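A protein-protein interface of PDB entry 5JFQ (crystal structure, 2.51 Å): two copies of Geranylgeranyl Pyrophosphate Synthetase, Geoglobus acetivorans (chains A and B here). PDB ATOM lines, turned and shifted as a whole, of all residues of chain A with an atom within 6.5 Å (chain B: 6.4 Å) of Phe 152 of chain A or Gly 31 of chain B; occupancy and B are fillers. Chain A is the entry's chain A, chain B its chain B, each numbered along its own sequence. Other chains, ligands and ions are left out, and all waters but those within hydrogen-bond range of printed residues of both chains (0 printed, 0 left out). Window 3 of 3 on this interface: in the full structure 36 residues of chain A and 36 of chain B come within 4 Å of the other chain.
The side-chain carboxylate of Glu 149 of chain A lies within hydrogen-bond range of the side-chain amide nitrogen of Gln 27 of chain B, 3.1 Å away.
The side-chain hydroxyl (OH) of Tyr 33 of chain B lies within hydrogen-bond range of the side-chain carboxylate (OE2) of Glu 149 of chain A.
Cys 148 of chain A touches Leu 32 of chain B (O to CD2, 3.8 Å).
O of Cys 148 of chain A touches CD1 of Leu 110 of chain B, 3.9 Å away.
CG of Glu 149 of chain A touches CD of Pro 29 of chain B (3.7 Å).
CD2 of Leu 32 of chain B touches N of Glu 149 of chain A, 3.8 Å away.
Gln 151 of chain A touches Leu 110 of chain B.
Phe 152 of chain A touches Pro 29 of chain B.
Gly 31 of chain B touches Phe 152 of chain A (CA to CZ, 3.7 Å).
Phe 152 of chain A touches Leu 32 of chain B.
Phe 152 of chain A touches Thr 107 of chain B (CE2 to OG1, 3.6 Å).
CD1 of Leu 110 of chain B touches CE of Met 155 of chain A, 3.6 Å away.
Phe 152 of chain A touches just these residues of chain B: Pro 29, Gly 31, Leu 32, Thr 107 and Leu 110.
Gly 31 of chain B touches just one residue of chain A: Phe 152 (3.7 Å).
Printed residues of chain A within 4 Å of Thr 107 of chain B: Phe 152 (3.6 Å).
Of the printed residues of chain A, Glu 28 of chain B touches Glu 149 (3.9 Å).
The nearest printed residue of chain A that does not touch Gly 31 of chain B is Ser 156 of chain A (8.6 Å).
Of the 13 printed residues of chain A, 5 touch a printed residue of chain B.
Printed residues of chain A that touch a printed residue of chain B: Cys 148, Glu 149, Gln 151, Phe 152 and Met 155.
Hydrophobic or aromatic side chains of chain A that line the printed part of chain B: Phe 152 and Met 155.
Of the 13 printed residues of chain B, 8 touch a printed residue of chain A.
Hydrophobic or aromatic side chains of chain B that line the printed part of chain A: Pro 29, Leu 32, Tyr 33 and Leu 110.
NZ of Lys 175 of chain A is in hydrogen-bond range of OE1 of Gln 151 of chain A, 2.8 Å away.
The side-chain carboxylate (OE2) of Glu 28 of chain B is in hydrogen-bond range of the backbone NH (N) of Glu 30 of chain B.
No position is printed for both chains.
Of the 14 pairs that touch across the chains among the printed residues, none has its exchanged pair printed and touching as well.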
ATOM      1  N   ILE A 147      -0.361  21.455 -14.471  1.00  0.00           N
ATOM      2  CA  ILE A 147       0.537  22.204 -13.616  1.00  0.00           C
ATOM      3  C   ILE A 147       0.820  23.567 -14.232  1.00  0.00           C
ATOM      4  O   ILE A 147       0.829  24.590 -13.536  1.00  0.00           O
ATOM      5  CB  ILE A 147       1.833  21.414 -13.381  1.00  0.00           C
ATOM      6  CG1 ILE A 147       1.517  20.051 -12.768  1.00  0.00           C
ATOM      7  CG2 ILE A 147       2.830  22.265 -12.532  1.00  0.00           C
ATOM      8  CD1 ILE A 147       2.732  19.158 -12.641  1.00  0.00           C
ATOM      9  N   CYS A 148       1.042  23.595 -15.552  1.00  0.00           N
ATOM     10  CA  CYS A 148       1.221  24.851 -16.261  1.00  0.00           C
ATOM     11  C   CYS A 148      -0.004  25.738 -16.118  1.00  0.00           C
ATOM     12  O   CYS A 148       0.116  26.953 -15.913  1.00  0.00           O
ATOM     13  CB  CYS A 148       1.515  24.578 -17.734  1.00  0.00           C
ATOM     14  SG  CYS A 148       2.990  23.578 -17.975  1.00  0.00           S
ATOM     15  N   GLU A 149      -1.195  25.154 -16.211  1.00  0.00           N
ATOM     16  CA  GLU A 149      -2.392  25.933 -15.924  1.00  0.00           C
ATOM     17  C   GLU A 149      -2.390  26.414 -14.480  1.00  0.00           C
ATOM     18  O   GLU A 149      -2.795  27.544 -14.191  1.00  0.00           O
ATOM     19  CB  GLU A 149      -3.645  25.111 -16.225  1.00  0.00           C
ATOM     20  CG  GLU A 149      -3.784  24.753 -17.676  1.00  0.00           C
ATOM     21  CD  GLU A 149      -4.769  23.637 -17.884  1.00  0.00           C
ATOM     22  OE1 GLU A 149      -5.327  23.190 -16.869  1.00  0.00           O
ATOM     23  OE2 GLU A 149      -4.987  23.225 -19.042  1.00  0.00           O
ATOM     24  N   GLY A 150      -1.943  25.568 -13.554  1.00  0.00           N
ATOM     25  CA  GLY A 150      -1.885  25.998 -12.173  1.00  0.00           C
ATOM     26  C   GLY A 150      -0.868  27.105 -11.983  1.00  0.00           C
ATOM     27  O   GLY A 150      -1.154  28.133 -11.356  1.00  0.00           O
ATOM     28  N   GLN A 151       0.334  26.913 -12.528  1.00  0.00           N
ATOM     29  CA  GLN A 151       1.350  27.949 -12.426  1.00  0.00           C
ATOM     30  C   GLN A 151       0.833  29.254 -13.022  1.00  0.00           C
ATOM     31  O   GLN A 151       0.953  30.318 -12.400  1.00  0.00           O
ATOM     32  CB  GLN A 151       2.635  27.474 -13.099  1.00  0.00           C
ATOM     33  CG  GLN A 151       3.797  28.460 -13.057  1.00  0.00           C
ATOM     34  CD  GLN A 151       4.119  28.961 -11.655  1.00  0.00           C
ATOM     35  OE1 GLN A 151       3.699  28.367 -10.646  1.00  0.00           O
ATOM     36  NE2 GLN A 151       4.858  30.072 -11.585  1.00  0.00           N
ATOM     37  N   PHE A 152       0.182  29.178 -14.191  1.00  0.00           N
ATOM     38  CA  PHE A 152      -0.392  30.373 -14.802  1.00  0.00           C
ATOM     39  C   PHE A 152      -1.385  31.054 -13.861  1.00  0.00           C
ATOM     40  O   PHE A 152      -1.323  32.272 -13.650  1.00  0.00           O
ATOM     41  CB  PHE A 152      -1.067  30.033 -16.136  1.00  0.00           C
ATOM     42  CG  PHE A 152      -1.586  31.233 -16.844  1.00  0.00           C
ATOM     43  CD1 PHE A 152      -2.877  31.678 -16.622  1.00  0.00           C
ATOM     44  CD2 PHE A 152      -0.759  31.974 -17.680  1.00  0.00           C
ATOM     45  CE1 PHE A 152      -3.349  32.824 -17.247  1.00  0.00           C
ATOM     46  CE2 PHE A 152      -1.225  33.119 -18.318  1.00  0.00           C
ATOM     47  CZ  PHE A 152      -2.518  33.544 -18.101  1.00  0.00           C
ATOM     48  N   MET A 153      -2.315  30.284 -13.299  1.00  0.00           N
ATOM     49  CA  MET A 153      -3.294  30.851 -12.378  1.00  0.00           C
ATOM     50  C   MET A 153      -2.593  31.538 -11.220  1.00  0.00           C
ATOM     51  O   MET A 153      -2.915  32.679 -10.865  1.00  0.00           O
ATOM     52  CB  MET A 153      -4.239  29.751 -11.856  1.00  0.00           C
ATOM     53  CG  MET A 153      -5.264  29.234 -12.867  1.00  0.00           C
ATOM     54  SD  MET A 153      -6.222  27.769 -12.297  1.00  0.00           S
ATOM     55  CE  MET A 153      -7.142  28.440 -10.891  1.00  0.00           C
ATOM     56  N   ASP A 154      -1.635  30.842 -10.611  1.00  0.00           N
ATOM     57  CA  ASP A 154      -0.927  31.390  -9.465  1.00  0.00           C
ATOM     58  C   ASP A 154      -0.322  32.757  -9.786  1.00  0.00           C
ATOM     59  O   ASP A 154      -0.413  33.691  -8.981  1.00  0.00           O
ATOM     60  CB  ASP A 154       0.152  30.408  -9.031  1.00  0.00           C
ATOM     61  CG  ASP A 154       0.667  30.699  -7.673  1.00  0.00           C
ATOM     62  OD1 ASP A 154      -0.121  31.189  -6.847  1.00  0.00           O
ATOM     63  OD2 ASP A 154       1.865  30.443  -7.428  1.00  0.00           O
ATOM     64  N   MET A 155       0.289  32.892 -10.964  1.00  0.00           N
ATOM     65  CA  MET A 155       0.837  34.181 -11.366  1.00  0.00           C
ATOM     66  C   MET A 155      -0.261  35.206 -11.571  1.00  0.00           C
ATOM     67  O   MET A 155      -0.111  36.361 -11.165  1.00  0.00           O
ATOM     68  CB  MET A 155       1.671  34.028 -12.629  1.00  0.00           C
ATOM     69  CG  MET A 155       3.061  33.491 -12.337  1.00  0.00           C
ATOM     70  SD  MET A 155       4.035  33.363 -13.831  1.00  0.00           S
ATOM     71  CE  MET A 155       2.764  33.031 -15.057  1.00  0.00           C
ATOM     72  N   SER A 156      -1.374  34.800 -12.188  1.00  0.00           N
ATOM     73  CA  SER A 156      -2.506  35.706 -12.319  1.00  0.00           C
ATOM     74  C   SER A 156      -2.894  36.252 -10.962  1.00  0.00           C
ATOM     75  O   SER A 156      -3.166  37.449 -10.815  1.00  0.00           O
ATOM     76  CB  SER A 156      -3.694  34.994 -12.981  1.00  0.00           C
ATOM     77  OG  SER A 156      -4.522  34.322 -12.035  1.00  0.00           O
ATOM     78  N   PHE A 157      -2.880  35.391  -9.947  1.00  0.00           N
ATOM     79  CA  PHE A 157      -3.259  35.827  -8.612  1.00  0.00           C
ATOM     80  C   PHE A 157      -2.360  36.953  -8.111  1.00  0.00           C
ATOM     81  O   PHE A 157      -2.813  37.805  -7.337  1.00  0.00           O
ATOM     82  CB  PHE A 157      -3.209  34.659  -7.632  1.00  0.00           C
ATOM     83  CG  PHE A 157      -4.299  33.647  -7.813  1.00  0.00           C
ATOM     84  CD1 PHE A 157      -5.202  33.735  -8.860  1.00  0.00           C
ATOM     85  CD2 PHE A 157      -4.415  32.588  -6.913  1.00  0.00           C
ATOM     86  CE1 PHE A 157      -6.201  32.784  -9.010  1.00  0.00           C
ATOM     87  CE2 PHE A 157      -5.405  31.634  -7.056  1.00  0.00           C
ATOM     88  CZ  PHE A 157      -6.303  31.735  -8.106  1.00  0.00           C
ATOM     89  N   MET A 171      -6.571  26.521  -8.002  1.00  0.00           N
ATOM     90  CA  MET A 171      -5.182  26.754  -8.364  1.00  0.00           C
ATOM     91  C   MET A 171      -4.269  25.724  -7.706  1.00  0.00           C
ATOM     92  O   MET A 171      -3.480  25.056  -8.384  1.00  0.00           O
ATOM     93  CB  MET A 171      -4.785  28.181  -7.973  1.00  0.00           C
ATOM     94  CG  MET A 171      -3.407  28.563  -8.375  1.00  0.00           C
ATOM     95  SD  MET A 171      -2.165  27.984  -7.220  1.00  0.00           S
ATOM     96  CE  MET A 171      -2.607  28.863  -5.725  1.00  0.00           C
ATOM     97  N   LYS A 175      -1.600  23.235  -9.325  1.00  0.00           N
ATOM     98  CA  LYS A 175      -0.214  23.615  -9.104  1.00  0.00           C
ATOM     99  C   LYS A 175       0.519  22.560  -8.282  1.00  0.00           C
ATOM    100  O   LYS A 175       1.672  22.225  -8.576  1.00  0.00           O
ATOM    101  CB  LYS A 175      -0.173  24.986  -8.422  1.00  0.00           C
ATOM    102  CG  LYS A 175       1.209  25.524  -8.170  1.00  0.00           C
ATOM    103  CD  LYS A 175       2.031  25.641  -9.444  1.00  0.00           C
ATOM    104  CE  LYS A 175       3.541  25.802  -9.123  1.00  0.00           C
ATOM    105  NZ  LYS A 175       4.382  25.624 -10.346  1.00  0.00           N
ATOM    106  N   GLN B  27      -8.496  26.829 -24.639  1.00  0.00           N
ATOM    107  CA  GLN B  27      -9.086  26.309 -23.414  1.00  0.00           C
ATOM    108  C   GLN B  27      -8.787  27.325 -22.308  1.00  0.00           C
ATOM    109  O   GLN B  27      -8.150  28.354 -22.552  1.00  0.00           O
ATOM    110  CB  GLN B  27      -8.523  24.907 -23.176  1.00  0.00           C
ATOM    111  CG  GLN B  27      -9.009  24.128 -21.987  1.00  0.00           C
ATOM    112  CD  GLN B  27      -8.052  22.984 -21.696  1.00  0.00           C
ATOM    113  OE1 GLN B  27      -7.573  22.327 -22.630  1.00  0.00           O
ATOM    114  NE2 GLN B  27      -7.726  22.768 -20.407  1.00  0.00           N
ATOM    115  N   GLU B  28      -9.307  27.050 -21.049  1.00  0.00           N
ATOM    116  CA  GLU B  28      -8.891  27.983 -20.008  1.00  0.00           C
ATOM    117  C   GLU B  28      -7.611  27.496 -19.335  1.00  0.00           C
ATOM    118  O   GLU B  28      -7.312  26.304 -19.358  1.00  0.00           O
ATOM    119  CB  GLU B  28      -9.984  28.140 -18.961  1.00  0.00           C
ATOM    120  CG  GLU B  28     -11.109  29.083 -19.372  1.00  0.00           C
ATOM    121  CD  GLU B  28     -10.722  30.559 -19.228  1.00  0.00           C
ATOM    122  OE1 GLU B  28     -11.411  31.423 -19.824  1.00  0.00           O
ATOM    123  OE2 GLU B  28      -9.734  30.859 -18.511  1.00  0.00           O
ATOM    124  N   PRO B  29      -6.773  28.383 -18.765  1.00  0.00           N
ATOM    125  CA  PRO B  29      -6.803  29.855 -18.800  1.00  0.00           C
ATOM    126  C   PRO B  29      -6.552  30.373 -20.212  1.00  0.00           C
ATOM    127  O   PRO B  29      -5.511  30.012 -20.792  1.00  0.00           O
ATOM    128  CB  PRO B  29      -5.658  30.260 -17.868  1.00  0.00           C
ATOM    129  CG  PRO B  29      -5.319  29.052 -17.087  1.00  0.00           C
ATOM    130  CD  PRO B  29      -5.637  27.887 -17.971  1.00  0.00           C
ATOM    131  N   GLU B  30      -7.472  31.180 -20.759  1.00  0.00           N
ATOM    132  CA  GLU B  30      -7.311  31.621 -22.143  1.00  0.00           C
ATOM    133  C   GLU B  30      -5.977  32.322 -22.346  1.00  0.00           C
ATOM    134  O   GLU B  30      -5.369  32.204 -23.413  1.00  0.00           O
ATOM    135  CB  GLU B  30      -8.454  32.539 -22.570  1.00  0.00           C
ATOM    136  CG  GLU B  30      -9.088  33.355 -21.486  1.00  0.00           C
ATOM    137  CD  GLU B  30     -10.313  34.113 -22.004  1.00  0.00           C
ATOM    138  OE1 GLU B  30     -10.333  34.457 -23.214  1.00  0.00           O
ATOM    139  OE2 GLU B  30     -11.263  34.345 -21.208  1.00  0.00           O
ATOM    140  N   GLY B  31      -5.507  33.059 -21.336  1.00  0.00           N
ATOM    141  CA  GLY B  31      -4.186  33.650 -21.437  1.00  0.00           C
ATOM    142  C   GLY B  31      -3.145  32.638 -21.861  1.00  0.00           C
ATOM    143  O   GLY B  31      -2.428  32.840 -22.842  1.00  0.00           O
ATOM    144  N   LEU B  32      -3.095  31.497 -21.164  1.00  0.00           N
ATOM    145  CA  LEU B  32      -2.083  30.485 -21.449  1.00  0.00           C
ATOM    146  C   LEU B  32      -2.275  29.874 -22.833  1.00  0.00           C
ATOM    147  O   LEU B  32      -1.300  29.632 -23.562  1.00  0.00           O
ATOM    148  CB  LEU B  32      -2.127  29.410 -20.366  1.00  0.00           C
ATOM    149  CG  LEU B  32      -1.160  28.240 -20.521  1.00  0.00           C
ATOM    150  CD1 LEU B  32       0.280  28.753 -20.582  1.00  0.00           C
ATOM    151  CD2 LEU B  32      -1.344  27.216 -19.394  1.00  0.00           C
ATOM    152  N   TYR B  33      -3.521  29.639 -23.224  1.00  0.00           N
ATOM    153  CA  TYR B  33      -3.759  28.950 -24.483  1.00  0.00           C
ATOM    154  C   TYR B  33      -3.727  29.901 -25.670  1.00  0.00           C
ATOM    155  O   TYR B  33      -3.357  29.487 -26.777  1.00  0.00           O
ATOM    156  CB  TYR B  33      -5.078  28.173 -24.401  1.00  0.00           C
ATOM    157  CG  TYR B  33      -4.911  26.892 -23.614  1.00  0.00           C
ATOM    158  CD1 TYR B  33      -5.132  26.854 -22.242  1.00  0.00           C
ATOM    159  CD2 TYR B  33      -4.465  25.734 -24.233  1.00  0.00           C
ATOM    160  CE1 TYR B  33      -4.953  25.683 -21.520  1.00  0.00           C
ATOM    161  CE2 TYR B  33      -4.280  24.555 -23.521  1.00  0.00           C
ATOM    162  CZ  TYR B  33      -4.530  24.534 -22.168  1.00  0.00           C
ATOM    163  OH  TYR B  33      -4.339  23.360 -21.465  1.00  0.00           O
ATOM    164  N   ARG B  34      -4.087  31.171 -25.466  1.00  0.00           N
ATOM    165  CA  ARG B  34      -3.898  32.156 -26.522  1.00  0.00           C
ATOM    166  C   ARG B  34      -2.435  32.187 -26.929  1.00  0.00           C
ATOM    167  O   ARG B  34      -2.108  32.171 -28.122  1.00  0.00           O
ATOM    168  CB  ARG B  34      -4.373  33.523 -26.034  1.00  0.00           C
ATOM    169  CG  ARG B  34      -5.048  34.421 -27.072  1.00  0.00           C
ATOM    170  CD  ARG B  34      -5.374  35.787 -26.438  1.00  0.00           C
ATOM    171  NE  ARG B  34      -6.160  35.635 -25.208  1.00  0.00           N
ATOM    172  CZ  ARG B  34      -6.095  36.453 -24.154  1.00  0.00           C
ATOM    173  NH1 ARG B  34      -5.254  37.493 -24.162  1.00  0.00           N
ATOM    174  NH2 ARG B  34      -6.868  36.221 -23.087  1.00  0.00           N
ATOM    175  N   ALA B  35      -1.544  32.147 -25.935  1.00  0.00           N
ATOM    176  CA  ALA B  35      -0.115  32.066 -26.193  1.00  0.00           C
ATOM    177  C   ALA B  35       0.269  30.722 -26.798  1.00  0.00           C
ATOM    178  O   ALA B  35       1.063  30.662 -27.745  1.00  0.00           O
ATOM    179  CB  ALA B  35       0.661  32.313 -24.896  1.00  0.00           C
ATOM    180  N   ALA B  36      -0.273  29.623 -26.262  1.00  0.00           N
ATOM    181  CA  ALA B  36       0.148  28.307 -26.744  1.00  0.00           C
ATOM    182  C   ALA B  36      -0.342  28.005 -28.152  1.00  0.00           C
ATOM    183  O   ALA B  36       0.229  27.143 -28.824  1.00  0.00           O
ATOM    184  CB  ALA B  36      -0.333  27.199 -25.804  1.00  0.00           C
ATOM    185  N   PHE B 103       2.910  38.201 -24.827  1.00  0.00           N
ATOM    186  CA  PHE B 103       2.337  37.698 -23.592  1.00  0.00           C
ATOM    187  C   PHE B 103       3.300  37.730 -22.428  1.00  0.00           C
ATOM    188  O   PHE B 103       2.867  37.562 -21.283  1.00  0.00           O
ATOM    189  CB  PHE B 103       1.850  36.255 -23.769  1.00  0.00           C
ATOM    190  CG  PHE B 103       1.095  36.020 -25.026  1.00  0.00           C
ATOM    191  CD1 PHE B 103      -0.288  36.161 -25.062  1.00  0.00           C
ATOM    192  CD2 PHE B 103       1.750  35.623 -26.172  1.00  0.00           C
ATOM    193  CE1 PHE B 103      -1.012  35.914 -26.227  1.00  0.00           C
ATOM    194  CE2 PHE B 103       1.038  35.377 -27.342  1.00  0.00           C
ATOM    195  CZ  PHE B 103      -0.349  35.526 -27.366  1.00  0.00           C
ATOM    196  N   THR B 107       4.664  33.609 -19.403  1.00  0.00           N
ATOM    197  CA  THR B 107       3.603  32.928 -20.141  1.00  0.00           C
ATOM    198  C   THR B 107       4.160  32.193 -21.353  1.00  0.00           C
ATOM    199  O   THR B 107       3.729  31.076 -21.657  1.00  0.00           O
ATOM    200  CB  THR B 107       2.516  33.911 -20.564  1.00  0.00           C
ATOM    201  OG1 THR B 107       1.936  34.509 -19.397  1.00  0.00           O
ATOM    202  CG2 THR B 107       1.419  33.192 -21.343  1.00  0.00           C
ATOM    203  N   LEU B 110       5.481  28.934 -20.047  1.00  0.00           N
ATOM    204  CA  LEU B 110       4.372  28.015 -19.788  1.00  0.00           C
ATOM    205  C   LEU B 110       3.696  27.568 -21.073  1.00  0.00           C
ATOM    206  O   LEU B 110       3.190  26.441 -21.141  1.00  0.00           O
ATOM    207  CB  LEU B 110       3.324  28.646 -18.862  1.00  0.00           C
ATOM    208  CG  LEU B 110       3.746  28.994 -17.426  1.00  0.00           C
ATOM    209  CD1 LEU B 110       2.663  29.788 -16.660  1.00  0.00           C
ATOM    210  CD2 LEU B 110       4.192  27.755 -16.660  1.00  0.00           C
